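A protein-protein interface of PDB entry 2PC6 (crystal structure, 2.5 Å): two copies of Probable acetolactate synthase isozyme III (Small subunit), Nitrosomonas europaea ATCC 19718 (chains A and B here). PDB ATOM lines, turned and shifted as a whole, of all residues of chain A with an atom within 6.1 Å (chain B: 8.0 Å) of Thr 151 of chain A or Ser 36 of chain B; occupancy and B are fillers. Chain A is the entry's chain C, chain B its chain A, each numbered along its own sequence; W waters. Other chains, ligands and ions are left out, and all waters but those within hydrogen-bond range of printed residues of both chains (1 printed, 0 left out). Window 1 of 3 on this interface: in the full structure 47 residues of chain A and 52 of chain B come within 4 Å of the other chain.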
ATOM      1  N   SER A  34      14.666 -15.464 -27.095  1.00  0.00           N
ATOM      2  CA  SER A  34      13.376 -15.194 -26.496  1.00  0.00           C
ATOM      3  C   SER A  34      12.752 -16.481 -25.962  1.00  0.00           C
ATOM      4  O   SER A  34      13.093 -17.589 -26.380  1.00  0.00           O
ATOM      5  CB  SER A  34      12.431 -14.541 -27.504  1.00  0.00           C
ATOM      6  OG  SER A  34      11.855 -15.519 -28.376  1.00  0.00           O
ATOM      7  N   LEU A  35      11.827 -16.314 -25.041  1.00  0.00           N
ATOM      8  CA  LEU A  35      11.263 -17.420 -24.356  1.00  0.00           C
ATOM      9  C   LEU A  35       9.928 -16.984 -23.747  1.00  0.00           C
ATOM     10  O   LEU A  35       9.775 -15.837 -23.227  1.00  0.00           O
ATOM     11  CB  LEU A  35      12.228 -17.944 -23.262  1.00  0.00           C
ATOM     12  CG  LEU A  35      11.814 -19.274 -22.605  1.00  0.00           C
ATOM     13  CD1 LEU A  35      12.974 -20.158 -22.208  1.00  0.00           C
ATOM     14  CD2 LEU A  35      10.835 -19.080 -21.401  1.00  0.00           C
ATOM     15  N   SER A  36       8.973 -17.913 -23.838  1.00  0.00           N
ATOM     16  CA  SER A  36       7.662 -17.745 -23.261  1.00  0.00           C
ATOM     17  C   SER A  36       7.296 -19.078 -22.690  1.00  0.00           C
ATOM     18  O   SER A  36       7.503 -20.118 -23.324  1.00  0.00           O
ATOM     19  CB  SER A  36       6.645 -17.383 -24.339  1.00  0.00           C
ATOM     20  OG  SER A  36       6.604 -15.989 -24.576  1.00  0.00           O
ATOM     21  N   VAL A  37       6.733 -19.054 -21.496  1.00  0.00           N
ATOM     22  CA  VAL A  37       6.179 -20.270 -20.933  1.00  0.00           C
ATOM     23  C   VAL A  37       4.950 -19.883 -20.098  1.00  0.00           C
ATOM     24  O   VAL A  37       4.981 -18.898 -19.327  1.00  0.00           O
ATOM     25  CB  VAL A  37       7.233 -21.010 -20.080  1.00  0.00           C
ATOM     26  CG1 VAL A  37       7.940 -20.034 -19.215  1.00  0.00           C
ATOM     27  CG2 VAL A  37       6.582 -22.087 -19.223  1.00  0.00           C
ATOM     28  N   ARG A  86       3.414 -16.229 -33.607  1.00  0.00           N
ATOM     29  CA  ARG A  86       3.077 -14.843 -33.380  1.00  0.00           C
ATOM     30  C   ARG A  86       3.834 -14.391 -32.155  1.00  0.00           C
ATOM     31  O   ARG A  86       3.993 -15.156 -31.176  1.00  0.00           O
ATOM     32  CB  ARG A  86       1.567 -14.699 -33.134  1.00  0.00           C
ATOM     33  CG  ARG A  86       0.669 -14.945 -34.332  1.00  0.00           C
ATOM     34  CD  ARG A  86       0.911 -13.897 -35.381  1.00  0.00           C
ATOM     35  NE  ARG A  86       0.030 -13.990 -36.521  1.00  0.00           N
ATOM     36  CZ  ARG A  86       0.234 -14.799 -37.563  1.00  0.00           C
ATOM     37  NH1 ARG A  86       1.263 -15.621 -37.585  1.00  0.00           N
ATOM     38  NH2 ARG A  86      -0.627 -14.830 -38.565  1.00  0.00           N
ATOM     39  N   GLU A  87       4.325 -13.155 -32.205  1.00  0.00           N
ATOM     40  CA  GLU A  87       4.676 -12.449 -30.972  1.00  0.00           C
ATOM     41  C   GLU A  87       3.864 -11.212 -30.799  1.00  0.00           C
ATOM     42  O   GLU A  87       3.295 -10.696 -31.731  1.00  0.00           O
ATOM     43  CB  GLU A  87       6.117 -12.033 -30.951  1.00  0.00           C
ATOM     44  CG  GLU A  87       7.020 -13.152 -31.226  1.00  0.00           C
ATOM     45  CD  GLU A  87       8.214 -12.702 -32.049  1.00  0.00           C
ATOM     46  OE1 GLU A  87       8.527 -13.389 -33.055  1.00  0.00           O
ATOM     47  OE2 GLU A  87       8.815 -11.660 -31.678  1.00  0.00           O
ATOM     48  N   LEU A  88       3.845 -10.780 -29.561  1.00  0.00           N
ATOM     49  CA  LEU A  88       3.283  -9.543 -29.086  1.00  0.00           C
ATOM     50  C   LEU A  88       4.386  -8.636 -28.564  1.00  0.00           C
ATOM     51  O   LEU A  88       5.378  -9.097 -27.985  1.00  0.00           O
ATOM     52  CB  LEU A  88       2.375  -9.849 -27.912  1.00  0.00           C
ATOM     53  CG  LEU A  88       2.122  -8.712 -26.905  1.00  0.00           C
ATOM     54  CD1 LEU A  88       1.038  -7.804 -27.397  1.00  0.00           C
ATOM     55  CD2 LEU A  88       1.713  -9.340 -25.578  1.00  0.00           C
ATOM     56  N   MET A  89       4.181  -7.351 -28.762  1.00  0.00           N
ATOM     57  CA  MET A  89       5.107  -6.326 -28.351  1.00  0.00           C
ATOM     58  C   MET A  89       4.368  -5.075 -27.884  1.00  0.00           C
ATOM     59  O   MET A  89       3.353  -4.695 -28.459  1.00  0.00           O
ATOM     60  CB  MET A  89       5.986  -5.976 -29.530  1.00  0.00           C
ATOM     61  CG  MET A  89       7.207  -5.272 -29.162  1.00  0.00           C
ATOM     62  SD  MET A  89       8.301  -4.770 -30.708  1.00  0.00           S
ATOM     63  CE  MET A  89       7.128  -3.717 -31.887  1.00  0.00           C
ATOM     64  N   ALA A 149       8.604  -3.825 -24.380  1.00  0.00           N
ATOM     65  CA  ALA A 149       8.495  -5.149 -23.773  1.00  0.00           C
ATOM     66  C   ALA A 149       7.878  -6.089 -24.752  1.00  0.00           C
ATOM     67  O   ALA A 149       6.735  -5.930 -25.176  1.00  0.00           O
ATOM     68  CB  ALA A 149       7.711  -5.133 -22.476  1.00  0.00           C
ATOM     69  N   ARG A 150       8.655  -7.083 -25.119  1.00  0.00           N
ATOM     70  CA  ARG A 150       8.347  -7.934 -26.261  1.00  0.00           C
ATOM     71  C   ARG A 150       8.361  -9.363 -25.757  1.00  0.00           C
ATOM     72  O   ARG A 150       9.270  -9.717 -25.006  1.00  0.00           O
ATOM     73  CB  ARG A 150       9.395  -7.690 -27.323  1.00  0.00           C
ATOM     74  CG  ARG A 150       9.540  -8.766 -28.372  1.00  0.00           C
ATOM     75  CD  ARG A 150      10.644  -8.356 -29.274  1.00  0.00           C
ATOM     76  NE  ARG A 150      10.517  -9.025 -30.541  1.00  0.00           N
ATOM     77  CZ  ARG A 150      10.896  -8.510 -31.714  1.00  0.00           C
ATOM     78  NH1 ARG A 150      11.431  -7.283 -31.813  1.00  0.00           N
ATOM     79  NH2 ARG A 150      10.746  -9.241 -32.799  1.00  0.00           N
ATOM     80  N   THR A 151       7.374 -10.182 -26.151  1.00  0.00           N
ATOM     81  CA  THR A 151       7.210 -11.532 -25.557  1.00  0.00           C
ATOM     82  C   THR A 151       7.965 -12.705 -26.139  1.00  0.00           C
ATOM     83  O   THR A 151       8.044 -13.761 -25.496  1.00  0.00           O
ATOM     84  CB  THR A 151       5.787 -12.012 -25.470  1.00  0.00           C
ATOM     85  OG1 THR A 151       5.270 -12.250 -26.794  1.00  0.00           O
ATOM     86  CG2 THR A 151       4.946 -11.049 -24.658  1.00  0.00           C
ATOM     87  N   GLY A 152       8.523 -12.591 -27.326  1.00  0.00           N
ATOM     88  CA  GLY A 152       9.073 -13.840 -27.876  1.00  0.00           C
ATOM     89  C   GLY A 152       7.971 -14.840 -28.233  1.00  0.00           C
ATOM     90  O   GLY A 152       6.834 -14.714 -27.768  1.00  0.00           O
ATOM     91  N   VAL A 153       8.302 -15.821 -29.069  1.00  0.00           N
ATOM     92  CA  VAL A 153       7.299 -16.561 -29.816  1.00  0.00           C
ATOM     93  C   VAL A 153       6.288 -17.389 -29.033  1.00  0.00           C
ATOM     94  O   VAL A 153       6.555 -17.882 -27.948  1.00  0.00           O
ATOM     95  CB  VAL A 153       7.942 -17.426 -30.870  1.00  0.00           C
ATOM     96  CG1 VAL A 153       6.856 -18.301 -31.601  1.00  0.00           C
ATOM     97  CG2 VAL A 153       8.726 -16.531 -31.842  1.00  0.00           C
ATOM     98  N   SER A 154       5.097 -17.460 -29.581  1.00  0.00           N
ATOM     99  CA  SER A 154       4.087 -18.424 -29.216  1.00  0.00           C
ATOM    100  C   SER A 154       3.752 -19.183 -30.545  1.00  0.00           C
ATOM    101  O   SER A 154       3.283 -18.592 -31.514  1.00  0.00           O
ATOM    102  CB  SER A 154       2.869 -17.655 -28.684  1.00  0.00           C
ATOM    103  OG  SER A 154       1.636 -18.371 -28.829  1.00  0.00           O
ATOM    104  N   ILE B   7       6.216  -8.884 -11.813  1.00  0.00           N
ATOM    105  CA  ILE B   7       7.584  -8.384 -11.746  1.00  0.00           C
ATOM    106  C   ILE B   7       8.186  -8.167 -13.164  1.00  0.00           C
ATOM    107  O   ILE B   7       8.099  -9.030 -14.067  1.00  0.00           O
ATOM    108  CB  ILE B   7       8.464  -9.302 -10.897  1.00  0.00           C
ATOM    109  CG1 ILE B   7       8.213  -9.021  -9.417  1.00  0.00           C
ATOM    110  CG2 ILE B   7       9.888  -9.015 -11.137  1.00  0.00           C
ATOM    111  CD1 ILE B   7       7.392 -10.036  -8.716  1.00  0.00           C
ATOM    112  N   SER B   8       8.779  -6.987 -13.319  1.00  0.00           N
ATOM    113  CA  SER B   8       9.400  -6.531 -14.535  1.00  0.00           C
ATOM    114  C   SER B   8      10.882  -6.318 -14.275  1.00  0.00           C
ATOM    115  O   SER B   8      11.266  -5.652 -13.302  1.00  0.00           O
ATOM    116  CB  SER B   8       8.814  -5.177 -14.862  1.00  0.00           C
ATOM    117  OG  SER B   8       8.451  -5.113 -16.220  1.00  0.00           O
ATOM    118  N   LEU B   9      11.736  -6.851 -15.134  1.00  0.00           N
ATOM    119  CA  LEU B   9      13.148  -6.633 -14.907  1.00  0.00           C
ATOM    120  C   LEU B   9      13.979  -6.534 -16.177  1.00  0.00           C
ATOM    121  O   LEU B   9      13.597  -7.041 -17.239  1.00  0.00           O
ATOM    122  CB  LEU B   9      13.715  -7.628 -13.885  1.00  0.00           C
ATOM    123  CG  LEU B   9      13.480  -9.127 -14.014  1.00  0.00           C
ATOM    124  CD1 LEU B   9      14.602  -9.659 -14.861  1.00  0.00           C
ATOM    125  CD2 LEU B   9      13.537  -9.816 -12.660  1.00  0.00           C
ATOM    126  N   LEU B  18      19.134 -16.406 -17.642  1.00  0.00           N
ATOM    127  CA  LEU B  18      17.777 -16.838 -17.343  1.00  0.00           C
ATOM    128  C   LEU B  18      17.791 -18.107 -16.502  1.00  0.00           C
ATOM    129  O   LEU B  18      16.926 -18.267 -15.609  1.00  0.00           O
ATOM    130  CB  LEU B  18      16.908 -17.026 -18.615  1.00  0.00           C
ATOM    131  CG  LEU B  18      15.652 -17.875 -18.307  1.00  0.00           C
ATOM    132  CD1 LEU B  18      14.633 -17.068 -17.486  1.00  0.00           C
ATOM    133  CD2 LEU B  18      14.984 -18.428 -19.549  1.00  0.00           C
ATOM    134  N   ILE B  32       6.315 -19.597 -10.255  1.00  0.00           N
ATOM    135  CA  ILE B  32       6.384 -18.799 -11.451  1.00  0.00           C
ATOM    136  C   ILE B  32       5.127 -19.137 -12.223  1.00  0.00           C
ATOM    137  O   ILE B  32       4.951 -20.254 -12.695  1.00  0.00           O
ATOM    138  CB  ILE B  32       7.639 -19.130 -12.318  1.00  0.00           C
ATOM    139  CG1 ILE B  32       8.897 -18.668 -11.598  1.00  0.00           C
ATOM    140  CG2 ILE B  32       7.542 -18.427 -13.673  1.00  0.00           C
ATOM    141  CD1 ILE B  32      10.173 -18.833 -12.378  1.00  0.00           C
ATOM    142  N   SER B  34       3.996 -17.519 -14.975  1.00  0.00           N
ATOM    143  CA  SER B  34       4.287 -17.312 -16.384  1.00  0.00           C
ATOM    144  C   SER B  34       5.526 -16.403 -16.538  1.00  0.00           C
ATOM    145  O   SER B  34       5.847 -15.616 -15.653  1.00  0.00           O
ATOM    146  CB  SER B  34       3.071 -16.695 -17.080  1.00  0.00           C
ATOM    147  OG  SER B  34       3.090 -15.287 -16.958  1.00  0.00           O
ATOM    148  N   LEU B  35       6.189 -16.477 -17.676  1.00  0.00           N
ATOM    149  CA  LEU B  35       7.409 -15.745 -17.841  1.00  0.00           C
ATOM    150  C   LEU B  35       7.622 -15.354 -19.311  1.00  0.00           C
ATOM    151  O   LEU B  35       7.653 -16.221 -20.163  1.00  0.00           O
ATOM    152  CB  LEU B  35       8.591 -16.602 -17.351  1.00  0.00           C
ATOM    153  CG  LEU B  35       9.958 -15.924 -17.395  1.00  0.00           C
ATOM    154  CD1 LEU B  35      10.832 -16.343 -16.233  1.00  0.00           C
ATOM    155  CD2 LEU B  35      10.669 -16.216 -18.728  1.00  0.00           C
ATOM    156  N   SER B  36       7.838 -14.062 -19.560  1.00  0.00           N
ATOM    157  CA  SER B  36       8.249 -13.524 -20.845  1.00  0.00           C
ATOM    158  C   SER B  36       9.599 -12.851 -20.764  1.00  0.00           C
ATOM    159  O   SER B  36       9.828 -12.038 -19.880  1.00  0.00           O
ATOM    160  CB  SER B  36       7.292 -12.420 -21.249  1.00  0.00           C
ATOM    161  OG  SER B  36       6.562 -12.822 -22.359  1.00  0.00           O
ATOM    162  N   VAL B  37      10.468 -13.118 -21.726  1.00  0.00           N
ATOM    163  CA  VAL B  37      11.728 -12.405 -21.820  1.00  0.00           C
ATOM    164  C   VAL B  37      12.100 -12.264 -23.313  1.00  0.00           C
ATOM    165  O   VAL B  37      11.843 -13.155 -24.099  1.00  0.00           O
ATOM    166  CB  VAL B  37      12.825 -13.137 -20.989  1.00  0.00           C
ATOM    167  CG1 VAL B  37      13.040 -14.566 -21.480  1.00  0.00           C
ATOM    168  CG2 VAL B  37      14.134 -12.380 -21.002  1.00  0.00           C
ATOM    169  N   ALA B  38      12.651 -11.134 -23.713  1.00  0.00           N
ATOM    170  CA  ALA B  38      13.114 -10.915 -25.097  1.00  0.00           C
ATOM    171  C   ALA B  38      13.974  -9.669 -25.090  1.00  0.00           C
ATOM    172  O   ALA B  38      13.915  -8.906 -24.134  1.00  0.00           O
ATOM    173  CB  ALA B  38      11.930 -10.767 -26.091  1.00  0.00           C
ATOM    174  N   PRO B  39      14.799  -9.469 -26.134  1.00  0.00           N
ATOM    175  CA  PRO B  39      15.734  -8.324 -26.089  1.00  0.00           C
ATOM    176  C   PRO B  39      15.006  -6.992 -26.101  1.00  0.00           C
ATOM    177  O   PRO B  39      13.883  -6.907 -26.607  1.00  0.00           O
ATOM    178  CB  PRO B  39      16.563  -8.474 -27.404  1.00  0.00           C
ATOM    179  CG  PRO B  39      16.414  -9.928 -27.806  1.00  0.00           C
ATOM    180  CD  PRO B  39      14.945 -10.241 -27.390  1.00  0.00           C
ATOM    181  N   SER B  46      17.895  -7.560 -21.874  1.00  0.00           N
ATOM    182  CA  SER B  46      16.581  -8.130 -22.137  1.00  0.00           C
ATOM    183  C   SER B  46      15.602  -7.692 -21.078  1.00  0.00           C
ATOM    184  O   SER B  46      15.997  -7.315 -19.986  1.00  0.00           O
ATOM    185  CB  SER B  46      16.681  -9.659 -22.176  1.00  0.00           C
ATOM    186  OG  SER B  46      17.349 -10.098 -23.361  1.00  0.00           O
ATOM    187  N   ARG B  47      14.319  -7.746 -21.408  1.00  0.00           N
ATOM    188  CA  ARG B  47      13.254  -7.298 -20.508  1.00  0.00           C
ATOM    189  C   ARG B  47      12.450  -8.516 -20.131  1.00  0.00           C
ATOM    190  O   ARG B  47      11.950  -9.258 -20.968  1.00  0.00           O
ATOM    191  CB  ARG B  47      12.367  -6.243 -21.199  1.00  0.00           C
ATOM    192  CG  ARG B  47      11.063  -5.834 -20.468  1.00  0.00           C
ATOM    193  CD  ARG B  47      11.366  -4.790 -19.425  1.00  0.00           C
ATOM    194  NE  ARG B  47      10.201  -4.289 -18.679  1.00  0.00           N
ATOM    195  CZ  ARG B  47       9.759  -3.031 -18.726  1.00  0.00           C
ATOM    196  NH1 ARG B  47      10.337  -2.134 -19.512  1.00  0.00           N
ATOM    197  NH2 ARG B  47       8.731  -2.660 -17.988  1.00  0.00           N
ATOM    198  N   MET B  48      12.352  -8.759 -18.849  1.00  0.00           N
ATOM    199  CA  MET B  48      11.618  -9.914 -18.434  1.00  0.00           C
ATOM    200  C   MET B  48      10.400  -9.461 -17.705  1.00  0.00           C
ATOM    201  O   MET B  48      10.459  -8.553 -16.870  1.00  0.00           O
ATOM    202  CB  MET B  48      12.457 -10.784 -17.528  1.00  0.00           C
ATOM    203  CG  MET B  48      11.732 -12.016 -17.034  1.00  0.00           C
ATOM    204  SD  MET B  48      12.951 -13.175 -15.966  1.00  0.00           S
ATOM    205  CE  MET B  48      14.389 -13.488 -17.336  1.00  0.00           C
ATOM    206  N   THR B  49       9.298 -10.120 -18.021  1.00  0.00           N
ATOM    207  CA  THR B  49       8.094  -9.951 -17.270  1.00  0.00           C
ATOM    208  C   THR B  49       7.752 -11.303 -16.678  1.00  0.00           C
ATOM    209  O   THR B  49       7.505 -12.261 -17.399  1.00  0.00           O
ATOM    210  CB  THR B  49       6.936  -9.455 -18.151  1.00  0.00           C
ATOM    211  OG1 THR B  49       7.355  -8.278 -18.859  1.00  0.00           O
ATOM    212  CG2 THR B  49       5.769  -9.135 -17.298  1.00  0.00           C
ATOM    213  N   LEU B  50       7.711 -11.341 -15.364  1.00  0.00           N
ATOM    214  CA  LEU B  50       7.443 -12.531 -14.661  1.00  0.00           C
ATOM    215  C   LEU B  50       6.216 -12.358 -13.733  1.00  0.00           C
ATOM    216  O   LEU B  50       6.068 -11.327 -13.054  1.00  0.00           O
ATOM    217  CB  LEU B  50       8.682 -12.798 -13.836  1.00  0.00           C
ATOM    218  CG  LEU B  50       8.792 -14.069 -13.050  1.00  0.00           C
ATOM    219  CD1 LEU B  50      10.246 -14.166 -12.727  1.00  0.00           C
ATOM    220  CD2 LEU B  50       7.951 -13.959 -11.771  1.00  0.00           C
ATOM    221  N   VAL B  51       5.340 -13.355 -13.703  1.00  0.00           N
ATOM    222  CA  VAL B  51       4.194 -13.305 -12.816  1.00  0.00           C
ATOM    223  C   VAL B  51       4.395 -14.337 -11.731  1.00  0.00           C
ATOM    224  O   VAL B  51       4.666 -15.498 -12.019  1.00  0.00           O
ATOM    225  CB  VAL B  51       2.873 -13.632 -13.545  1.00  0.00           C
ATOM    226  CG1 VAL B  51       1.736 -13.757 -12.549  1.00  0.00           C
ATOM    227  CG2 VAL B  51       2.577 -12.598 -14.598  1.00  0.00           C
ATOM    228  N   ARG B  86      -0.625  -7.032 -21.610  1.00  0.00           N
ATOM    229  CA  ARG B  86      -1.217  -7.782 -22.703  1.00  0.00           C
ATOM    230  C   ARG B  86      -0.606  -9.129 -22.768  1.00  0.00           C
ATOM    231  O   ARG B  86       0.548  -9.325 -22.401  1.00  0.00           O
ATOM    232  CB  ARG B  86      -1.060  -7.073 -24.057  1.00  0.00           C
ATOM    233  CG  ARG B  86      -1.881  -5.779 -24.172  1.00  0.00           C
ATOM    234  CD  ARG B  86      -3.356  -6.041 -23.986  1.00  0.00           C
ATOM    235  NE  ARG B  86      -4.172  -4.845 -24.292  1.00  0.00           N
ATOM    236  CZ  ARG B  86      -4.451  -3.911 -23.383  1.00  0.00           C
ATOM    237  NH1 ARG B  86      -3.965  -4.062 -22.160  1.00  0.00           N
ATOM    238  NH2 ARG B  86      -5.184  -2.821 -23.680  1.00  0.00           N
ATOM    239  N   GLU B  87      -1.404 -10.082 -23.205  1.00  0.00           N
ATOM    240  CA  GLU B  87      -0.878 -11.383 -23.460  1.00  0.00           C
ATOM    241  C   GLU B  87      -1.346 -11.814 -24.822  1.00  0.00           C
ATOM    242  O   GLU B  87      -2.415 -11.388 -25.281  1.00  0.00           O
ATOM    243  CB  GLU B  87      -1.424 -12.323 -22.411  1.00  0.00           C
ATOM    244  CG  GLU B  87      -0.671 -13.649 -22.355  1.00  0.00           C
ATOM    245  CD  GLU B  87      -1.141 -14.487 -21.168  1.00  0.00           C
ATOM    246  OE1 GLU B  87      -2.012 -13.980 -20.370  1.00  0.00           O
ATOM    247  OE2 GLU B  87      -0.635 -15.638 -21.038  1.00  0.00           O
ATOM    248  N   LEU B  88      -0.554 -12.649 -25.474  1.00  0.00           N
ATOM    249  CA  LEU B  88      -0.999 -13.295 -26.705  1.00  0.00           C
ATOM    250  C   LEU B  88      -1.202 -14.797 -26.512  1.00  0.00           C
ATOM    251  O   LEU B  88      -0.454 -15.470 -25.812  1.00  0.00           O
ATOM    252  CB  LEU B  88      -0.035 -13.004 -27.871  1.00  0.00           C
ATOM    253  CG  LEU B  88      -0.402 -13.595 -29.254  1.00  0.00           C
ATOM    254  CD1 LEU B  88       0.022 -12.674 -30.369  1.00  0.00           C
ATOM    255  CD2 LEU B  88       0.350 -14.857 -29.392  1.00  0.00           C
ATOM    256  N   ARG B 150       0.532 -19.770 -25.289  1.00  0.00           N
ATOM    257  CA  ARG B 150       0.120 -18.608 -24.582  1.00  0.00           C
ATOM    258  C   ARG B 150       1.413 -18.021 -24.096  1.00  0.00           C
ATOM    259  O   ARG B 150       2.211 -18.716 -23.458  1.00  0.00           O
ATOM    260  CB  ARG B 150      -0.772 -19.076 -23.446  1.00  0.00           C
ATOM    261  CG  ARG B 150      -1.091 -18.057 -22.409  1.00  0.00           C
ATOM    262  CD  ARG B 150      -2.134 -18.587 -21.457  1.00  0.00           C
ATOM    263  NE  ARG B 150      -2.639 -17.487 -20.655  1.00  0.00           N
ATOM    264  CZ  ARG B 150      -3.838 -17.475 -20.077  1.00  0.00           C
ATOM    265  NH1 ARG B 150      -4.653 -18.515 -20.220  1.00  0.00           N
ATOM    266  NH2 ARG B 150      -4.238 -16.413 -19.380  1.00  0.00           N
ATOM    267  N   THR B 151       1.634 -16.748 -24.434  1.00  0.00           N
ATOM    268  CA  THR B 151       2.968 -16.124 -24.370  1.00  0.00           C
ATOM    269  C   THR B 151       3.360 -15.651 -23.000  1.00  0.00           C
ATOM    270  O   THR B 151       4.512 -15.218 -22.822  1.00  0.00           O
ATOM    271  CB  THR B 151       3.129 -14.833 -25.216  1.00  0.00           C
ATOM    272  OG1 THR B 151       2.147 -13.857 -24.813  1.00  0.00           O
ATOM    273  CG2 THR B 151       3.047 -15.120 -26.658  1.00  0.00           C
ATOM    274  N   GLY B 152       2.423 -15.670 -22.052  1.00  0.00           N
ATOM    275  CA  GLY B 152       2.701 -15.015 -20.782  1.00  0.00           C
ATOM    276  C   GLY B 152       2.754 -13.499 -20.945  1.00  0.00           C
ATOM    277  O   GLY B 152       3.093 -12.976 -22.015  1.00  0.00           O
ATOM    278  N   VAL B 153       2.391 -12.809 -19.868  1.00  0.00           N
ATOM    279  CA  VAL B 153       2.179 -11.375 -19.858  1.00  0.00           C
ATOM    280  C   VAL B 153       3.373 -10.567 -20.310  1.00  0.00           C
ATOM    281  O   VAL B 153       4.532 -10.910 -20.071  1.00  0.00           O
ATOM    282  CB  VAL B 153       1.793 -10.869 -18.459  1.00  0.00           C
ATOM    283  CG1 VAL B 153       1.835  -9.332 -18.426  1.00  0.00           C
ATOM    284  CG2 VAL B 153       0.391 -11.352 -18.086  1.00  0.00           C
ATOM    285  N   SER B 154       3.073  -9.489 -20.989  1.00  0.00           N
ATOM    286  CA  SER B 154       4.046  -8.490 -21.222  1.00  0.00           C
ATOM    287  C   SER B 154       3.445  -7.150 -20.759  1.00  0.00           C
ATOM    288  O   SER B 154       2.318  -6.812 -21.120  1.00  0.00           O
ATOM    289  CB  SER B 154       4.357  -8.475 -22.678  1.00  0.00           C
ATOM    290  OG  SER B 154       4.879  -7.205 -22.987  1.00  0.00           O
ATOM    291  N   GLY B 155       4.174  -6.416 -19.924  1.00  0.00           N
ATOM    292  CA  GLY B 155       3.666  -5.159 -19.379  1.00  0.00           C
ATOM    293  C   GLY B 155       4.624  -3.984 -19.354  1.00  0.00           C
ATOM    294  O   GLY B 155       5.856  -4.140 -19.401  1.00  0.00           O
HETATM  295  O   HOH W   1      11.883  -6.666 -24.860  1.00  0.00           O
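Thr 151 of chain A touches just these residues of chain B: Ser 36 (3.3 Å), Thr 151 (3.6 Å), Gly 152 (3.8 Å) and Ser 154 (3.3 Å). Ser 36 of chain B touches three residues of chain A. Of chain B, only Thr 151 (3.97 Å) comes within 4 Å of Gly 152 of chain A. Printed residues of chain A within 4 Å of Gly 155 of chain B: Ala 149. Of the printed residues of chain B, Val 37 of chain A touches Ser 34 (3.4 Å) and Leu 35 (3.2 Å). Printed residues of chain A within 4 Å of Val 37 of chain B: Ser 34 (3.5 Å) and Leu 35 (3.2 Å). Of the printed residues of chain B, Leu 35 of chain A touches Leu 18 (3.8 Å), Leu 35 (3.7 Å), Ser 36 (3.7 Å) and Val 37 (3.2 Å). Of the printed residues of chain A, Thr 151 of chain B touches Ser 36 (2.8 Å), Thr 151 (3.6 Å), Gly 152 (3.97 Å) and Ser 154 (3.3 Å). The nearest printed residue of chain B that does not touch Ser 34 of chain A is Ala 38 of chain B (4.1 Å).
Hydrophobic or aromatic side chains of chain A within 4 Å of the printed part of chain B: Leu 35, Val 37, Leu 88 and Ala 149. Of the 26 printed residues of chain B, 15 touch a printed residue of chain A. Hydrophobic or aromatic side chains of chain B that line the printed part of chain A: Leu 18, Leu 35, Val 37, Ala 38 and Leu 88. Along chain B the printed residues that touch a printed residue of chain A span positions 18 to 155. Among the printed residues, 26 pairs touch across the chains. Among the printed residues, no Asp or Glu carboxylate lies within 4 Å of a Lys or Arg side-chain nitrogen of the other chain.
Among the printed residues, pairs that only touch across the chains: Arg 150 of chain A with Ala 38 of chain B, Ser 154 of chain A with Thr 151 of chain B, Thr 151 of chain A with Ser 154 of chain B, Thr 151 of chain A with Ser 36 of chain B, Leu 88 of chain A with Arg 86 of chain B, Val 37 of chain A with Ser 34 of chain B, Ser 36 of chain A with Leu 35 of chain B, Ser 34 of chain A with Val 37 of chain B, Thr 151 of chain A with Thr 151 of chain B, Leu 35 of chain A with Ser 36 of chain B, Ala 149 of chain A with Gly 155 of chain B, Leu 35 of chain A with Leu 35 of chain B, Leu 35 of chain A with Leu 18 of chain B, Thr 151 of chain A with Gly 152 of chain B, Arg 86 of chain A with Leu 88 of chain B, Ser 154 of chain A with Leu 88 of chain B, Ser 36 of chain A with Ser 36 of chain B, Leu 88 of chain A with Glu 87 of chain B, Ser 154 of chain A with Arg 150 of chain B, Gly 152 of chain A with Thr 151 of chain B, Ala 149 of chain A with Arg 47 of chain B and Leu 88 of chain A with Leu 88 of chain B.
The backbone carbonyl oxygen (O) of Ser 36 of chain B lies within hydrogen-bond range of the backbone NH (N) of Thr 49 of chain B. The backbone NH of Ser 154 of chain B sits at hydrogen-bond distance from the backbone carbonyl oxygen of Arg 86 of chain B. O of Gly 152 of chain B lies within hydrogen-bond range of OG of Ser 36 of chain B (3.5 Å). OE2 of Glu 87 of chain B is in hydrogen-bond range of N of Gly 152 of chain B (3.2 Å). The backbone carbonyl oxygen of Ser 34 of chain B sits at hydrogen-bond distance from the backbone NH of Val 51 of chain B, 3.0 Å away.
O of Thr 151 of chain B is in hydrogen-bond range of OG of Ser 36 of chain A (2.8 Å). OG of Ser 154 of chain B lies within hydrogen-bond range of O of Ala 149 of chain A, 3.1 Å away. O of Val 37 of chain A lies within hydrogen-bond range of N of Leu 35 of chain B. N of Val 37 of chain B is in hydrogen-bond range of O of Leu 35 of chain A, 3.2 Å away.
Water W1 lies within hydrogen-bond range of O of Pro 39 of chain B, O of Ala 38 of chain B and N of Arg 150 of chain A.
Leu 35 of chain A touches Ser 36 of chain B, and with the chains exchanged Ser 36 of chain A touches Leu 35 of chain B. Leu 88 of chain B touches its own counterpart, Leu 88 of chain A. Thr 151 of chain A touches Gly 152 of chain B, and with the chains exchanged Gly 152 of chain A touches Thr 151 of chain B. Of the 26 pairs that touch across the chains among the printed residues, 18 have their exchanged pair printed and touching as well.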
